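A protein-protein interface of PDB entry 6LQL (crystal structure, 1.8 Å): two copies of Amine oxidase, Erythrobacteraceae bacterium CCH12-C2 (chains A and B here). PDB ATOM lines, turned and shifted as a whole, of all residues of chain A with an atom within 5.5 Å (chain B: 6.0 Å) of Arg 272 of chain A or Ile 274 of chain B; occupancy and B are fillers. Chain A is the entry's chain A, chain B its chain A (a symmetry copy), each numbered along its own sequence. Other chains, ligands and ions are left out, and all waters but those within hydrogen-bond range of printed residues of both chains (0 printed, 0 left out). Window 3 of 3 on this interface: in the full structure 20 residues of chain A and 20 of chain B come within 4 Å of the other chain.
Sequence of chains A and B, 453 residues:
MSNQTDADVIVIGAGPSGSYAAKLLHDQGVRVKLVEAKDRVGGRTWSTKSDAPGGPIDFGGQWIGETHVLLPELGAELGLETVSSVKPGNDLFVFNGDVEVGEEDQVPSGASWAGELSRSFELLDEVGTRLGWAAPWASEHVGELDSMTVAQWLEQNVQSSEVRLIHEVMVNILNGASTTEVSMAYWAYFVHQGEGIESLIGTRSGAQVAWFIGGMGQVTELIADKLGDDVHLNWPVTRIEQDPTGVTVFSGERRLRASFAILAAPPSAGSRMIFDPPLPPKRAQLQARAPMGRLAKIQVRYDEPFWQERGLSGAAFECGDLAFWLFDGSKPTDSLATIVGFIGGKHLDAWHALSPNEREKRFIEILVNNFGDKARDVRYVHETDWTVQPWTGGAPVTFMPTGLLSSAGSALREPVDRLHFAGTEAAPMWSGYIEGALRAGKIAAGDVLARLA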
ATOM      1  N   THR A 238      12.967 -15.985 -13.244  1.00  0.00           N
ATOM      2  CA  THR A 238      13.376 -17.067 -12.361  1.00  0.00           C
ATOM      3  C   THR A 238      14.492 -17.927 -12.937  1.00  0.00           C
ATOM      4  O   THR A 238      15.128 -18.672 -12.184  1.00  0.00           O
ATOM      5  CB  THR A 238      12.174 -17.966 -12.038  1.00  0.00           C
ATOM      6  OG1 THR A 238      11.527 -18.325 -13.270  1.00  0.00           O
ATOM      7  CG2 THR A 238      11.174 -17.219 -11.170  1.00  0.00           C
ATOM      8  N   SER A 268      22.449  -9.217  -5.960  1.00  0.00           N
ATOM      9  CA  SER A 268      21.546  -9.990  -5.114  1.00  0.00           C
ATOM     10  C   SER A 268      20.296 -10.437  -5.871  1.00  0.00           C
ATOM     11  O   SER A 268      19.749 -11.500  -5.568  1.00  0.00           O
ATOM     12  CB  SER A 268      21.135  -9.175  -3.877  1.00  0.00           C
ATOM     13  OG  SER A 268      20.660  -7.867  -4.203  1.00  0.00           O
ATOM     14  N   ALA A 269      19.814  -9.634  -6.823  1.00  0.00           N
ATOM     15  CA  ALA A 269      18.680 -10.070  -7.643  1.00  0.00           C
ATOM     16  C   ALA A 269      19.062 -11.254  -8.525  1.00  0.00           C
ATOM     17  O   ALA A 269      18.277 -12.191  -8.694  1.00  0.00           O
ATOM     18  CB  ALA A 269      18.168  -8.907  -8.495  1.00  0.00           C
ATOM     19  N   GLY A 270      20.264 -11.233  -9.090  1.00  0.00           N
ATOM     20  CA  GLY A 270      20.718 -12.369  -9.872  1.00  0.00           C
ATOM     21  C   GLY A 270      20.854 -13.640  -9.058  1.00  0.00           C
ATOM     22  O   GLY A 270      20.666 -14.744  -9.574  1.00  0.00           O
ATOM     23  N   SER A 271      21.186 -13.514  -7.772  1.00  0.00           N
ATOM     24  CA  SER A 271      21.409 -14.722  -6.986  1.00  0.00           C
ATOM     25  C   SER A 271      20.150 -15.572  -6.852  1.00  0.00           C
ATOM     26  O   SER A 271      20.257 -16.773  -6.586  1.00  0.00           O
ATOM     27  CB  SER A 271      21.931 -14.360  -5.589  1.00  0.00           C
ATOM     28  OG  SER A 271      20.876 -13.785  -4.822  1.00  0.00           O
ATOM     29  N   ARG A 272      18.960 -14.989  -7.013  1.00  0.00           N
ATOM     30  CA  ARG A 272      17.728 -15.759  -6.904  1.00  0.00           C
ATOM     31  C   ARG A 272      17.384 -16.518  -8.177  1.00  0.00           C
ATOM     32  O   ARG A 272      16.493 -17.364  -8.140  1.00  0.00           O
ATOM     33  CB  ARG A 272      16.553 -14.841  -6.541  1.00  0.00           C
ATOM     34  CG  ARG A 272      16.969 -13.406  -6.324  1.00  0.00           C
ATOM     35  CD  ARG A 272      17.233 -13.107  -4.851  1.00  0.00           C
ATOM     36  NE  ARG A 272      15.995 -12.976  -4.084  1.00  0.00           N
ATOM     37  CZ  ARG A 272      14.998 -12.153  -4.396  1.00  0.00           C
ATOM     38  NH1 ARG A 272      15.080 -11.393  -5.480  1.00  0.00           N
ATOM     39  NH2 ARG A 272      13.919 -12.088  -3.620  1.00  0.00           N
ATOM     40  N   MET A 273      18.057 -16.239  -9.288  1.00  0.00           N
ATOM     41  CA  MET A 273      17.769 -16.894 -10.558  1.00  0.00           C
ATOM     42  C   MET A 273      18.603 -18.154 -10.717  1.00  0.00           C
ATOM     43  O   MET A 273      19.695 -18.273 -10.159  1.00  0.00           O
ATOM     44  CB  MET A 273      18.064 -15.946 -11.720  1.00  0.00           C
ATOM     45  CG  MET A 273      17.418 -14.602 -11.589  1.00  0.00           C
ATOM     46  SD  MET A 273      18.014 -13.469 -12.839  1.00  0.00           S
ATOM     47  CE  MET A 273      17.145 -11.984 -12.390  1.00  0.00           C
ATOM     48  N   ILE A 274      18.072 -19.104 -11.492  1.00  0.00           N
ATOM     49  CA  ILE A 274      18.814 -20.293 -11.900  1.00  0.00           C
ATOM     50  C   ILE A 274      19.403 -20.029 -13.276  1.00  0.00           C
ATOM     51  O   ILE A 274      18.691 -19.592 -14.186  1.00  0.00           O
ATOM     52  CB  ILE A 274      17.913 -21.542 -11.921  1.00  0.00           C
ATOM     53  CG1 ILE A 274      17.350 -21.844 -10.528  1.00  0.00           C
ATOM     54  CG2 ILE A 274      18.679 -22.742 -12.476  1.00  0.00           C
ATOM     55  CD1 ILE A 274      18.411 -22.083  -9.453  1.00  0.00           C
ATOM     56  N   PRO A 390       9.366  -6.115  -2.366  1.00  0.00           N
ATOM     57  CA  PRO A 390       9.655  -7.398  -3.010  1.00  0.00           C
ATOM     58  C   PRO A 390      10.540  -7.210  -4.234  1.00  0.00           C
ATOM     59  O   PRO A 390      10.367  -6.269  -5.011  1.00  0.00           O
ATOM     60  CB  PRO A 390       8.255  -7.924  -3.383  1.00  0.00           C
ATOM     61  CG  PRO A 390       7.455  -6.694  -3.577  1.00  0.00           C
ATOM     62  CD  PRO A 390       7.940  -5.761  -2.480  1.00  0.00           C
ATOM     63  N   TRP A 391      11.498  -8.124  -4.393  1.00  0.00           N
ATOM     64  CA  TRP A 391      12.502  -8.140  -5.460  1.00  0.00           C
ATOM     65  C   TRP A 391      13.482  -6.973  -5.374  1.00  0.00           C
ATOM     66  O   TRP A 391      14.272  -6.748  -6.311  1.00  0.00           O
ATOM     67  CB  TRP A 391      11.871  -8.190  -6.856  1.00  0.00           C
ATOM     68  CG  TRP A 391      11.029  -9.422  -7.068  1.00  0.00           C
ATOM     69  CD1 TRP A 391      11.472 -10.672  -7.305  1.00  0.00           C
ATOM     70  CD2 TRP A 391       9.597  -9.492  -7.052  1.00  0.00           C
ATOM     71  NE1 TRP A 391      10.406 -11.541  -7.428  1.00  0.00           N
ATOM     72  CE2 TRP A 391       9.244 -10.834  -7.275  1.00  0.00           C
ATOM     73  CE3 TRP A 391       8.589  -8.546  -6.872  1.00  0.00           C
ATOM     74  CZ2 TRP A 391       7.913 -11.257  -7.343  1.00  0.00           C
ATOM     75  CZ3 TRP A 391       7.262  -8.963  -6.925  1.00  0.00           C
ATOM     76  CH2 TRP A 391       6.941 -10.310  -7.159  1.00  0.00           C
ATOM     77  N   THR B 238       8.654 -20.470  -4.897  1.00  0.00           N
ATOM     78  CA  THR B 238       8.983 -19.095  -5.240  1.00  0.00           C
ATOM     79  C   THR B 238       8.287 -18.069  -4.358  1.00  0.00           C
ATOM     80  O   THR B 238       8.705 -16.906  -4.342  1.00  0.00           O
ATOM     81  CB  THR B 238       8.620 -18.818  -6.706  1.00  0.00           C
ATOM     82  OG1 THR B 238       7.269 -19.251  -6.932  1.00  0.00           O
ATOM     83  CG2 THR B 238       9.537 -19.598  -7.635  1.00  0.00           C
ATOM     84  N   ARG B 239       7.260 -18.466  -3.619  1.00  0.00           N
ATOM     85  CA  ARG B 239       6.490 -17.511  -2.841  1.00  0.00           C
ATOM     86  C   ARG B 239       5.792 -18.247  -1.713  1.00  0.00           C
ATOM     87  O   ARG B 239       5.322 -19.370  -1.900  1.00  0.00           O
ATOM     88  CB  ARG B 239       5.473 -16.791  -3.735  1.00  0.00           C
ATOM     89  CG  ARG B 239       4.392 -16.049  -2.959  1.00  0.00           C
ATOM     90  CD  ARG B 239       3.378 -15.429  -3.924  1.00  0.00           C
ATOM     91  NE  ARG B 239       4.016 -14.360  -4.656  1.00  0.00           N
ATOM     92  CZ  ARG B 239       3.893 -13.075  -4.349  1.00  0.00           C
ATOM     93  NH1 ARG B 239       3.118 -12.691  -3.344  1.00  0.00           N
ATOM     94  NH2 ARG B 239       4.542 -12.180  -5.073  1.00  0.00           N
ATOM     95  N   ILE B 240       5.764 -17.624  -0.534  1.00  0.00           N
ATOM     96  CA  ILE B 240       5.010 -18.125   0.608  1.00  0.00           C
ATOM     97  C   ILE B 240       4.090 -17.010   1.095  1.00  0.00           C
ATOM     98  O   ILE B 240       4.554 -15.911   1.425  1.00  0.00           O
ATOM     99  CB  ILE B 240       5.924 -18.625   1.742  1.00  0.00           C
ATOM    100  CG1 ILE B 240       6.812 -19.762   1.219  1.00  0.00           C
ATOM    101  CG2 ILE B 240       5.079 -19.104   2.924  1.00  0.00           C
ATOM    102  CD1 ILE B 240       7.745 -20.361   2.253  1.00  0.00           C
ATOM    103  N   GLU B 241       2.791 -17.288   1.136  1.00  0.00           N
ATOM    104  CA  GLU B 241       1.804 -16.348   1.645  1.00  0.00           C
ATOM    105  C   GLU B 241       1.171 -16.927   2.896  1.00  0.00           C
ATOM    106  O   GLU B 241       0.871 -18.120   2.949  1.00  0.00           O
ATOM    107  CB  GLU B 241       0.725 -16.071   0.594  1.00  0.00           C
ATOM    108  CG  GLU B 241       1.281 -15.372  -0.660  1.00  0.00           C
ATOM    109  CD  GLU B 241       0.208 -15.036  -1.688  1.00  0.00           C
ATOM    110  OE1 GLU B 241      -0.930 -15.523  -1.542  1.00  0.00           O
ATOM    111  OE2 GLU B 241       0.504 -14.287  -2.643  1.00  0.00           O
ATOM    112  N   GLY B 270      15.811 -19.491   1.499  1.00  0.00           N
ATOM    113  CA  GLY B 270      14.685 -18.621   1.791  1.00  0.00           C
ATOM    114  C   GLY B 270      14.817 -17.244   1.172  1.00  0.00           C
ATOM    115  O   GLY B 270      13.819 -16.611   0.822  1.00  0.00           O
ATOM    116  N   SER B 271      16.047 -16.750   1.026  1.00  0.00           N
ATOM    117  CA  SER B 271      16.201 -15.393   0.514  1.00  0.00           C
ATOM    118  C   SER B 271      15.687 -15.246  -0.913  1.00  0.00           C
ATOM    119  O   SER B 271      15.372 -14.127  -1.331  1.00  0.00           O
ATOM    120  CB  SER B 271      17.673 -14.964   0.573  1.00  0.00           C
ATOM    121  OG  SER B 271      18.412 -15.664  -0.424  1.00  0.00           O
ATOM    122  N   ARG B 272      15.603 -16.335  -1.682  1.00  0.00           N
ATOM    123  CA  ARG B 272      15.109 -16.249  -3.050  1.00  0.00           C
ATOM    124  C   ARG B 272      13.590 -16.229  -3.137  1.00  0.00           C
ATOM    125  O   ARG B 272      13.062 -15.945  -4.210  1.00  0.00           O
ATOM    126  CB  ARG B 272      15.638 -17.423  -3.885  1.00  0.00           C
ATOM    127  CG  ARG B 272      16.576 -18.321  -3.114  1.00  0.00           C
ATOM    128  CD  ARG B 272      18.036 -17.936  -3.328  1.00  0.00           C
ATOM    129  NE  ARG B 272      18.533 -18.361  -4.636  1.00  0.00           N
ATOM    130  CZ  ARG B 272      18.467 -19.606  -5.100  1.00  0.00           C
ATOM    131  NH1 ARG B 272      17.903 -20.557  -4.368  1.00  0.00           N
ATOM    132  NH2 ARG B 272      18.969 -19.899  -6.297  1.00  0.00           N
ATOM    133  N   MET B 273      12.885 -16.520  -2.049  1.00  0.00           N
ATOM    134  CA  MET B 273      11.428 -16.558  -2.053  1.00  0.00           C
ATOM    135  C   MET B 273      10.852 -15.195  -1.706  1.00  0.00           C
ATOM    136  O   MET B 273      11.479 -14.394  -1.009  1.00  0.00           O
ATOM    137  CB  MET B 273      10.923 -17.588  -1.044  1.00  0.00           C
ATOM    138  CG  MET B 273      11.549 -18.941  -1.190  1.00  0.00           C
ATOM    139  SD  MET B 273      11.111 -20.011   0.175  1.00  0.00           S
ATOM    140  CE  MET B 273      12.036 -21.474  -0.233  1.00  0.00           C
ATOM    141  N   ILE B 274       9.640 -14.937  -2.203  1.00  0.00           N
ATOM    142  CA  ILE B 274       8.866 -13.760  -1.818  1.00  0.00           C
ATOM    143  C   ILE B 274       7.909 -14.170  -0.711  1.00  0.00           C
ATOM    144  O   ILE B 274       7.197 -15.171  -0.840  1.00  0.00           O
ATOM    145  CB  ILE B 274       8.096 -13.174  -3.017  1.00  0.00           C
ATOM    146  CG1 ILE B 274       9.054 -12.715  -4.122  1.00  0.00           C
ATOM    147  CG2 ILE B 274       7.194 -12.028  -2.561  1.00  0.00           C
ATOM    148  CD1 ILE B 274      10.065 -11.654  -3.685  1.00  0.00           C
ATOM    149  N   PHE B 275       7.881 -13.400   0.372  1.00  0.00           N
ATOM    150  CA  PHE B 275       7.015 -13.670   1.512  1.00  0.00           C
ATOM    151  C   PHE B 275       5.955 -12.588   1.599  1.00  0.00           C
ATOM    152  O   PHE B 275       6.275 -11.399   1.539  1.00  0.00           O
ATOM    153  CB  PHE B 275       7.823 -13.721   2.815  1.00  0.00           C
ATOM    154  CG  PHE B 275       8.811 -14.838   2.845  1.00  0.00           C
ATOM    155  CD1 PHE B 275      10.029 -14.718   2.218  1.00  0.00           C
ATOM    156  CD2 PHE B 275       8.508 -16.025   3.464  1.00  0.00           C
ATOM    157  CE1 PHE B 275      10.922 -15.774   2.232  1.00  0.00           C
ATOM    158  CE2 PHE B 275       9.409 -17.080   3.495  1.00  0.00           C
ATOM    159  CZ  PHE B 275      10.609 -16.956   2.880  1.00  0.00           C
ATOM    160  N   ASP B 276       4.697 -13.000   1.718  1.00  0.00           N
ATOM    161  CA  ASP B 276       3.627 -12.027   1.914  1.00  0.00           C
ATOM    162  C   ASP B 276       2.663 -12.545   2.974  1.00  0.00           C
ATOM    163  O   ASP B 276       1.954 -13.536   2.745  1.00  0.00           O
ATOM    164  CB  ASP B 276       2.898 -11.742   0.601  1.00  0.00           C
ATOM    165  CG  ASP B 276       1.817 -10.694   0.760  1.00  0.00           C
ATOM    166  OD1 ASP B 276       1.695 -10.147   1.874  1.00  0.00           O
ATOM    167  OD2 ASP B 276       1.101 -10.427  -0.224  1.00  0.00           O
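Ser 271 of chain A touches Arg 272 of chain B, and with the chains exchanged Arg 272 of chain A touches Ser 271 of chain B. Arg 272 of chain B touches its own counterpart, Arg 272 of chain A. Arg 272 of chain A touches Ile 274 of chain B, and with the chains exchanged Ile 274 of chain A touches Arg 272 of chain B. Of the 7 pairs that touch across the chains among the printed residues, 5 have their exchanged pair printed and touching as well.
CA of Arg 272 of chain A touches NE of Arg 272 of chain B (3.5 Å). Arg 272 of chain A touches Ile 274 of chain B (NH2 to CD1, 3.9 Å). Ile 274 of chain A touches Arg 272 of chain B. CH2 of Trp 391 of chain A touches NH2 of Arg 239 of chain B, at 3.7 Å. CG1 of Ile 274 of chain B touches CE2 of Trp 391 of chain A, 3.7 Å away.
The backbone NH (N) of Ile 274 of chain B is in hydrogen-bond range of the backbone carbonyl oxygen (O) of Thr 238 of chain B, at 3.1 Å. N of Ile 240 of chain B lies within hydrogen-bond range of O of Ile 274 of chain B, 2.9 Å away. N of Ile 274 of chain A sits at hydrogen-bond distance from O of Thr 238 of chain A, at 3.1 Å. The side-chain hydroxyl (OG) of Ser 271 of chain A sits at hydrogen-bond distance from the backbone carbonyl oxygen (O) of Ser 268 of chain A, at 2.7 Å. The guanidinium group (NH1) of Arg 239 of chain B lies within salt-bridge range of the side-chain carboxylate (OE2) of Glu 241 of chain B, 3.1 Å away.
Of the 11 printed residues of chain B, 4 touch a printed residue of chain A. Hydrophobic or aromatic side chains of chain B within 4 Å of the printed part of chain A: Ile 274. Printed residues of chain A that touch a printed residue of chain B: Ser 271, Arg 272, Ile 274 and Trp 391. Along chain A the printed residues that touch a printed residue of chain B span positions 271 to 391.
Of chain B, only Ser 271, Arg 272 and Ile 274 come within 4 Å of Arg 272 of chain A. Of chain A, only Arg 272 (3.9 Å) and Trp 391 (3.7 Å) come within 4 Å of Ile 274 of chain B. Of the printed residues of chain A, Arg 272 of chain B touches Ser 271 (3.0 Å), Arg 272 (3.5 Å) and Ile 274 (3.9 Å). Of the printed residues of chain B, Ser 271 of chain A touches Arg 272 (3.0 Å). Printed residues of chain A within 4 Å of Arg 239 of chain B: Trp 391 (3.7 Å). Thr 238 of chain A touches none of the printed residues of chain B. The nearest residue of chain B that does not touch Arg 272 of chain A is Met 273 of chain B (4.3 Å). The nearest residue of chain A that does not touch Ile 274 of chain B is Pro 390 of chain A (4.2 Å). The nearest printed residue of chain A that does not touch Arg 239 of chain B is Pro 390 of chain A (5.9 Å).
The backbone carbonyl oxygen of Ser 271 of chain B sits at hydrogen-bond distance from the guanidinium group of Arg 272 of chain A (3.0 Å). O of Ser 271 of chain A sits at hydrogen-bond distance from NE of Arg 272 of chain B.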
